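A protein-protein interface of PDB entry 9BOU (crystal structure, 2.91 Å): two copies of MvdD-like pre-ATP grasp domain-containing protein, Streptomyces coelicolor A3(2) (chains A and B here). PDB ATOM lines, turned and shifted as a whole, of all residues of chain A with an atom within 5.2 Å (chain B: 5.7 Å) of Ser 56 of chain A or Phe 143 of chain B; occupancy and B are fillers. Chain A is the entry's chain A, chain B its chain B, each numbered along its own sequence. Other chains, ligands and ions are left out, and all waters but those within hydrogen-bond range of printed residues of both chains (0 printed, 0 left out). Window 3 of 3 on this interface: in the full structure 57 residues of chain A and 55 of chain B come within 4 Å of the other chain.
The backbone carbonyl oxygen of Ser 43 of chain A is in hydrogen-bond range of the backbone NH of His 54 of chain A.
OG1 of Thr 141 of chain B sits at hydrogen-bond distance from N of Phe 143 of chain B.
O of Val 188 of chain B sits close to OG1 of Thr 142 of chain B (3.5 Å).
The backbone NH of Ala 41 of chain A sits at hydrogen-bond distance from the backbone carbonyl oxygen of Ser 56 of chain A, at 2.9 Å.
Among the printed residues, pairs that only touch across the chains: Ala 41 of chain A with Thr 142 of chain B (3.4 Å), Ser 56 of chain A with Phe 143 of chain B (3.8 Å), Ser 43 of chain A with Phe 143 of chain B (3.8 Å), Leu 42 of chain A with Phe 143 of chain B (3.9 Å) and Ser 43 of chain A with Ala 146 of chain B (3.9 Å).
The side-chain hydroxyl (OG1) of Thr 141 of chain B sits close to the backbone carbonyl oxygen (O) of Leu 42 of chain A (3.4 Å).
The backbone carbonyl oxygen (O) of Leu 42 of chain A lies within hydrogen-bond range of the backbone NH (N) of Thr 142 of chain B (2.9 Å).
The side-chain hydroxyl (OG) of Ser 43 of chain A lies close to the side-chain hydroxyl (OG1) of Thr 141 of chain B, at 3.5 Å.
Hydrophobic or aromatic side chains of chain B within 4 Å of the printed part of chain A: Phe 143 and Ala 146.
Among the printed residues, 8 pairs touch across the chains.
Ser 56 of chain A touches one residue of chain B.
Phe 143 of chain B touches just these residues of chain A: Leu 42 (3.9 Å), Ser 43 (3.8 Å) and Ser 56 (3.8 Å).
Of the printed residues of chain A, Thr 141 of chain B touches Leu 42 and Ser 43.
Of the printed residues of chain B, Leu 42 of chain A touches Thr 141, Thr 142 and Phe 143.
Printed residues of chain B within 4 Å of Ser 43 of chain A: Thr 141, Phe 143 and Ala 146.
Arg 148 of chain B touches none of the printed residues of chain A.
The nearest printed residue of chain B that does not touch Ser 56 of chain A is Thr 142 of chain B (8.0 Å).
The nearest printed residue of chain A that does not touch Ala 146 of chain B is Leu 42 of chain A (6.6 Å).
No position is printed for both chains.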
ATOM      1  N   SER A  39     -19.169  12.247  13.834  1.00  0.00           N
ATOM      2  CA  SER A  39     -20.137  11.231  13.428  1.00  0.00           C
ATOM      3  C   SER A  39     -20.225  11.049  11.908  1.00  0.00           C
ATOM      4  O   SER A  39     -20.591   9.955  11.455  1.00  0.00           O
ATOM      5  CB  SER A  39     -21.483  11.643  14.063  1.00  0.00           C
ATOM      6  OG  SER A  39     -22.625  11.281  13.308  1.00  0.00           O
ATOM      7  N   VAL A  40     -19.848  12.057  11.117  1.00  0.00           N
ATOM      8  CA  VAL A  40     -20.105  12.109   9.681  1.00  0.00           C
ATOM      9  C   VAL A  40     -18.762  12.271   8.966  1.00  0.00           C
ATOM     10  O   VAL A  40     -17.880  12.998   9.441  1.00  0.00           O
ATOM     11  CB  VAL A  40     -21.072  13.273   9.350  1.00  0.00           C
ATOM     12  CG1 VAL A  40     -21.401  13.295   7.900  1.00  0.00           C
ATOM     13  CG2 VAL A  40     -22.384  13.194  10.138  1.00  0.00           C
ATOM     14  N   ALA A  41     -18.583  11.576   7.842  1.00  0.00           N
ATOM     15  CA  ALA A  41     -17.329  11.731   7.109  1.00  0.00           C
ATOM     16  C   ALA A  41     -17.558  11.363   5.662  1.00  0.00           C
ATOM     17  O   ALA A  41     -18.553  10.731   5.323  1.00  0.00           O
ATOM     18  CB  ALA A  41     -16.201  10.881   7.679  1.00  0.00           C
ATOM     19  N   LEU A  42     -16.605  11.741   4.813  1.00  0.00           N
ATOM     20  CA  LEU A  42     -16.814  11.703   3.372  1.00  0.00           C
ATOM     21  C   LEU A  42     -15.517  11.439   2.625  1.00  0.00           C
ATOM     22  O   LEU A  42     -14.426  11.633   3.160  1.00  0.00           O
ATOM     23  CB  LEU A  42     -17.389  13.027   2.868  1.00  0.00           C
ATOM     24  CG  LEU A  42     -16.630  14.243   3.376  1.00  0.00           C
ATOM     25  CD1 LEU A  42     -15.186  14.318   2.888  1.00  0.00           C
ATOM     26  CD2 LEU A  42     -17.319  15.534   2.972  1.00  0.00           C
ATOM     27  N   SER A  43     -15.648  11.028   1.359  1.00  0.00           N
ATOM     28  CA  SER A  43     -14.513  10.828   0.452  1.00  0.00           C
ATOM     29  C   SER A  43     -15.040  10.900  -0.977  1.00  0.00           C
ATOM     30  O   SER A  43     -16.053  10.275  -1.302  1.00  0.00           O
ATOM     31  CB  SER A  43     -13.789   9.477   0.668  1.00  0.00           C
ATOM     32  OG  SER A  43     -13.079   9.046  -0.488  1.00  0.00           O
ATOM     33  N   HIS A  54     -18.389   8.929  -1.518  1.00  0.00           N
ATOM     34  CA  HIS A  54     -19.219   8.252  -0.518  1.00  0.00           C
ATOM     35  C   HIS A  54     -19.448   9.098   0.730  1.00  0.00           C
ATOM     36  O   HIS A  54     -18.644   9.963   1.082  1.00  0.00           O
ATOM     37  CB  HIS A  54     -18.586   6.913  -0.068  1.00  0.00           C
ATOM     38  CG  HIS A  54     -18.637   5.862  -1.123  1.00  0.00           C
ATOM     39  ND1 HIS A  54     -17.847   5.910  -2.255  1.00  0.00           N
ATOM     40  CD2 HIS A  54     -19.438   4.777  -1.263  1.00  0.00           C
ATOM     41  CE1 HIS A  54     -18.154   4.894  -3.042  1.00  0.00           C
ATOM     42  NE2 HIS A  54     -19.117   4.193  -2.466  1.00  0.00           N
ATOM     43  N   LEU A  55     -20.543   8.796   1.433  1.00  0.00           N
ATOM     44  CA  LEU A  55     -20.880   9.439   2.705  1.00  0.00           C
ATOM     45  C   LEU A  55     -21.096   8.413   3.808  1.00  0.00           C
ATOM     46  O   LEU A  55     -21.641   7.344   3.552  1.00  0.00           O
ATOM     47  CB  LEU A  55     -22.136  10.233   2.560  1.00  0.00           C
ATOM     48  CG  LEU A  55     -22.045  11.506   1.745  1.00  0.00           C
ATOM     49  CD1 LEU A  55     -23.456  12.114   1.638  1.00  0.00           C
ATOM     50  CD2 LEU A  55     -21.069  12.445   2.403  1.00  0.00           C
ATOM     51  N   SER A  56     -20.704   8.748   5.033  1.00  0.00           N
ATOM     52  CA  SER A  56     -20.761   7.822   6.168  1.00  0.00           C
ATOM     53  C   SER A  56     -21.287   8.570   7.387  1.00  0.00           C
ATOM     54  O   SER A  56     -20.681   9.559   7.819  1.00  0.00           O
ATOM     55  CB  SER A  56     -19.361   7.231   6.433  1.00  0.00           C
ATOM     56  OG  SER A  56     -19.277   6.562   7.681  1.00  0.00           O
ATOM     57  N   SER A  57     -22.457   8.142   7.891  1.00  0.00           N
ATOM     58  CA  SER A  57     -23.003   8.624   9.157  1.00  0.00           C
ATOM     59  C   SER A  57     -23.264   7.392   9.999  1.00  0.00           C
ATOM     60  O   SER A  57     -23.789   6.392   9.494  1.00  0.00           O
ATOM     61  CB  SER A  57     -24.295   9.441   9.039  1.00  0.00           C
ATOM     62  OG  SER A  57     -24.486  10.225  10.212  1.00  0.00           O
ATOM     63  N   GLY A  58     -22.909   7.460  11.273  1.00  0.00           N
ATOM     64  CA  GLY A  58     -22.753   6.234  12.028  1.00  0.00           C
ATOM     65  C   GLY A  58     -21.922   5.296  11.186  1.00  0.00           C
ATOM     66  O   GLY A  58     -20.806   5.635  10.765  1.00  0.00           O
ATOM     67  N   GLY A  59     -22.477   4.125  10.900  1.00  0.00           N
ATOM     68  CA  GLY A  59     -21.804   3.145  10.069  1.00  0.00           C
ATOM     69  C   GLY A  59     -22.427   3.119   8.693  1.00  0.00           C
ATOM     70  O   GLY A  59     -21.834   2.626   7.732  1.00  0.00           O
ATOM     71  N   ARG A  60     -23.639   3.659   8.598  1.00  0.00           N
ATOM     72  CA  ARG A  60     -24.313   3.835   7.314  1.00  0.00           C
ATOM     73  C   ARG A  60     -23.369   4.449   6.272  1.00  0.00           C
ATOM     74  O   ARG A  60     -22.623   5.385   6.559  1.00  0.00           O
ATOM     75  CB  ARG A  60     -25.557   4.705   7.549  1.00  0.00           C
ATOM     76  CG  ARG A  60     -26.634   4.626   6.481  1.00  0.00           C
ATOM     77  CD  ARG A  60     -27.810   3.670   6.754  1.00  0.00           C
ATOM     78  NE  ARG A  60     -28.581   3.553   5.520  1.00  0.00           N
ATOM     79  CZ  ARG A  60     -28.082   3.084   4.379  1.00  0.00           C
ATOM     80  NH1 ARG A  60     -26.889   2.492   4.334  1.00  0.00           N
ATOM     81  NH2 ARG A  60     -28.784   3.231   3.250  1.00  0.00           N
ATOM     82  N   LEU A  61     -23.406   3.910   5.053  1.00  0.00           N
ATOM     83  CA  LEU A  61     -22.503   4.328   3.992  1.00  0.00           C
ATOM     84  C   LEU A  61     -23.225   4.255   2.652  1.00  0.00           C
ATOM     85  O   LEU A  61     -23.755   3.199   2.294  1.00  0.00           O
ATOM     86  CB  LEU A  61     -21.248   3.445   4.003  1.00  0.00           C
ATOM     87  CG  LEU A  61     -20.276   3.636   2.849  1.00  0.00           C
ATOM     88  CD1 LEU A  61     -19.151   4.577   3.261  1.00  0.00           C
ATOM     89  CD2 LEU A  61     -19.634   2.357   2.385  1.00  0.00           C
ATOM     90  N   THR B 141     -11.010  13.852   1.176  1.00  0.00           N
ATOM     91  CA  THR B 141     -11.468  12.770   2.026  1.00  0.00           C
ATOM     92  C   THR B 141     -11.264  13.042   3.502  1.00  0.00           C
ATOM     93  O   THR B 141     -10.596  13.984   3.896  1.00  0.00           O
ATOM     94  CB  THR B 141     -10.738  11.477   1.669  1.00  0.00           C
ATOM     95  OG1 THR B 141     -11.416  10.382   2.273  1.00  0.00           O
ATOM     96  CG2 THR B 141      -9.313  11.526   2.168  1.00  0.00           C
ATOM     97  N   THR B 142     -11.851  12.163   4.304  1.00  0.00           N
ATOM     98  CA  THR B 142     -11.740  12.124   5.754  1.00  0.00           C
ATOM     99  C   THR B 142     -11.491  10.705   6.239  1.00  0.00           C
ATOM    100  O   THR B 142     -11.322  10.502   7.437  1.00  0.00           O
ATOM    101  CB  THR B 142     -13.003  12.734   6.370  1.00  0.00           C
ATOM    102  OG1 THR B 142     -12.893  14.165   6.208  1.00  0.00           O
ATOM    103  CG2 THR B 142     -13.158  12.385   7.810  1.00  0.00           C
ATOM    104  N   PHE B 143     -11.390   9.729   5.326  1.00  0.00           N
ATOM    105  CA  PHE B 143     -10.894   8.393   5.648  1.00  0.00           C
ATOM    106  C   PHE B 143      -9.386   8.328   5.455  1.00  0.00           C
ATOM    107  O   PHE B 143      -8.919   8.376   4.308  1.00  0.00           O
ATOM    108  CB  PHE B 143     -11.557   7.336   4.766  1.00  0.00           C
ATOM    109  CG  PHE B 143     -13.016   7.225   4.961  1.00  0.00           C
ATOM    110  CD1 PHE B 143     -13.517   6.472   5.993  1.00  0.00           C
ATOM    111  CD2 PHE B 143     -13.892   7.901   4.131  1.00  0.00           C
ATOM    112  CE1 PHE B 143     -14.865   6.384   6.183  1.00  0.00           C
ATOM    113  CE2 PHE B 143     -15.241   7.817   4.320  1.00  0.00           C
ATOM    114  CZ  PHE B 143     -15.731   7.054   5.351  1.00  0.00           C
ATOM    115  N   PRO B 144      -8.595   8.204   6.515  1.00  0.00           N
ATOM    116  CA  PRO B 144      -7.168   7.910   6.325  1.00  0.00           C
ATOM    117  C   PRO B 144      -6.932   6.759   5.380  1.00  0.00           C
ATOM    118  O   PRO B 144      -5.967   6.777   4.609  1.00  0.00           O
ATOM    119  CB  PRO B 144      -6.700   7.582   7.740  1.00  0.00           C
ATOM    120  CG  PRO B 144      -7.602   8.413   8.597  1.00  0.00           C
ATOM    121  CD  PRO B 144      -8.933   8.482   7.920  1.00  0.00           C
ATOM    122  N   ARG B 145      -7.792   5.741   5.434  1.00  0.00           N
ATOM    123  CA  ARG B 145      -7.610   4.569   4.586  1.00  0.00           C
ATOM    124  C   ARG B 145      -7.716   4.951   3.114  1.00  0.00           C
ATOM    125  O   ARG B 145      -6.855   4.587   2.309  1.00  0.00           O
ATOM    126  CB  ARG B 145      -8.634   3.489   4.952  1.00  0.00           C
ATOM    127  CG  ARG B 145      -8.531   2.932   6.395  1.00  0.00           C
ATOM    128  CD  ARG B 145      -9.226   3.830   7.469  1.00  0.00           C
ATOM    129  NE  ARG B 145      -8.584   3.742   8.784  1.00  0.00           N
ATOM    130  CZ  ARG B 145      -8.981   4.413   9.859  1.00  0.00           C
ATOM    131  NH1 ARG B 145     -10.037   5.212   9.824  1.00  0.00           N
ATOM    132  NH2 ARG B 145      -8.303   4.278  10.997  1.00  0.00           N
ATOM    133  N   ALA B 146      -8.757   5.709   2.744  1.00  0.00           N
ATOM    134  CA  ALA B 146      -8.887   6.163   1.362  1.00  0.00           C
ATOM    135  C   ALA B 146      -7.687   6.989   0.939  1.00  0.00           C
ATOM    136  O   ALA B 146      -7.225   6.885  -0.197  1.00  0.00           O
ATOM    137  CB  ALA B 146     -10.158   6.988   1.177  1.00  0.00           C
ATOM    138  N   ALA B 147      -7.188   7.835   1.835  1.00  0.00           N
ATOM    139  CA  ALA B 147      -5.996   8.615   1.539  1.00  0.00           C
ATOM    140  C   ALA B 147      -4.809   7.703   1.270  1.00  0.00           C
ATOM    141  O   ALA B 147      -4.057   7.912   0.312  1.00  0.00           O
ATOM    142  CB  ALA B 147      -5.699   9.571   2.696  1.00  0.00           C
ATOM    143  N   ARG B 148      -4.629   6.673   2.105  1.00  0.00           N
ATOM    144  CA  ARG B 148      -3.452   5.812   1.983  1.00  0.00           C
ATOM    145  C   ARG B 148      -3.438   5.057   0.661  1.00  0.00           C
ATOM    146  O   ARG B 148      -2.379   4.895   0.044  1.00  0.00           O
ATOM    147  CB  ARG B 148      -3.422   4.814   3.135  1.00  0.00           C
ATOM    148  CG  ARG B 148      -2.444   5.083   4.252  1.00  0.00           C
ATOM    149  CD  ARG B 148      -2.773   4.139   5.447  1.00  0.00           C
ATOM    150  NE  ARG B 148      -3.203   4.854   6.648  1.00  0.00           N
ATOM    151  CZ  ARG B 148      -4.166   4.445   7.465  1.00  0.00           C
ATOM    152  NH1 ARG B 148      -4.819   3.316   7.249  1.00  0.00           N
ATOM    153  NH2 ARG B 148      -4.480   5.193   8.524  1.00  0.00           N
ATOM    154  N   PHE B 185      -1.555   9.648   6.865  1.00  0.00           N
ATOM    155  CA  PHE B 185      -2.826  10.263   6.504  1.00  0.00           C
ATOM    156  C   PHE B 185      -3.836  10.148   7.631  1.00  0.00           C
ATOM    157  O   PHE B 185      -5.048  10.159   7.382  1.00  0.00           O
ATOM    158  CB  PHE B 185      -3.399   9.654   5.204  1.00  0.00           C
ATOM    159  CG  PHE B 185      -2.482   9.772   4.005  1.00  0.00           C
ATOM    160  CD1 PHE B 185      -2.214  10.999   3.425  1.00  0.00           C
ATOM    161  CD2 PHE B 185      -1.898   8.640   3.453  1.00  0.00           C
ATOM    162  CE1 PHE B 185      -1.381  11.097   2.326  1.00  0.00           C
ATOM    163  CE2 PHE B 185      -1.053   8.737   2.359  1.00  0.00           C
ATOM    164  CZ  PHE B 185      -0.794   9.965   1.798  1.00  0.00           C
ATOM    165  N   VAL B 188      -6.380  13.071   8.500  1.00  0.00           N
ATOM    166  CA  VAL B 188      -7.454  13.410   7.578  1.00  0.00           C
ATOM    167  C   VAL B 188      -8.814  13.145   8.206  1.00  0.00           C
ATOM    168  O   VAL B 188      -9.813  13.755   7.789  1.00  0.00           O
ATOM    169  CB  VAL B 188      -7.251  12.633   6.255  1.00  0.00           C
ATOM    170  CG1 VAL B 188      -7.806  11.208   6.336  1.00  0.00           C
ATOM    171  CG2 VAL B 188      -7.875  13.409   5.091  1.00  0.00           C
ATOM    172  N   ALA B 189      -8.869  12.266   9.215  1.00  0.00           N
ATOM    173  CA  ALA B 189     -10.122  12.015   9.916  1.00  0.00           C
ATOM    174  C   ALA B 189     -10.660  13.281  10.576  1.00  0.00           C
ATOM    175  O   ALA B 189     -11.871  13.405  10.805  1.00  0.00           O
ATOM    176  CB  ALA B 189      -9.921  10.931  10.968  1.00  0.00           C
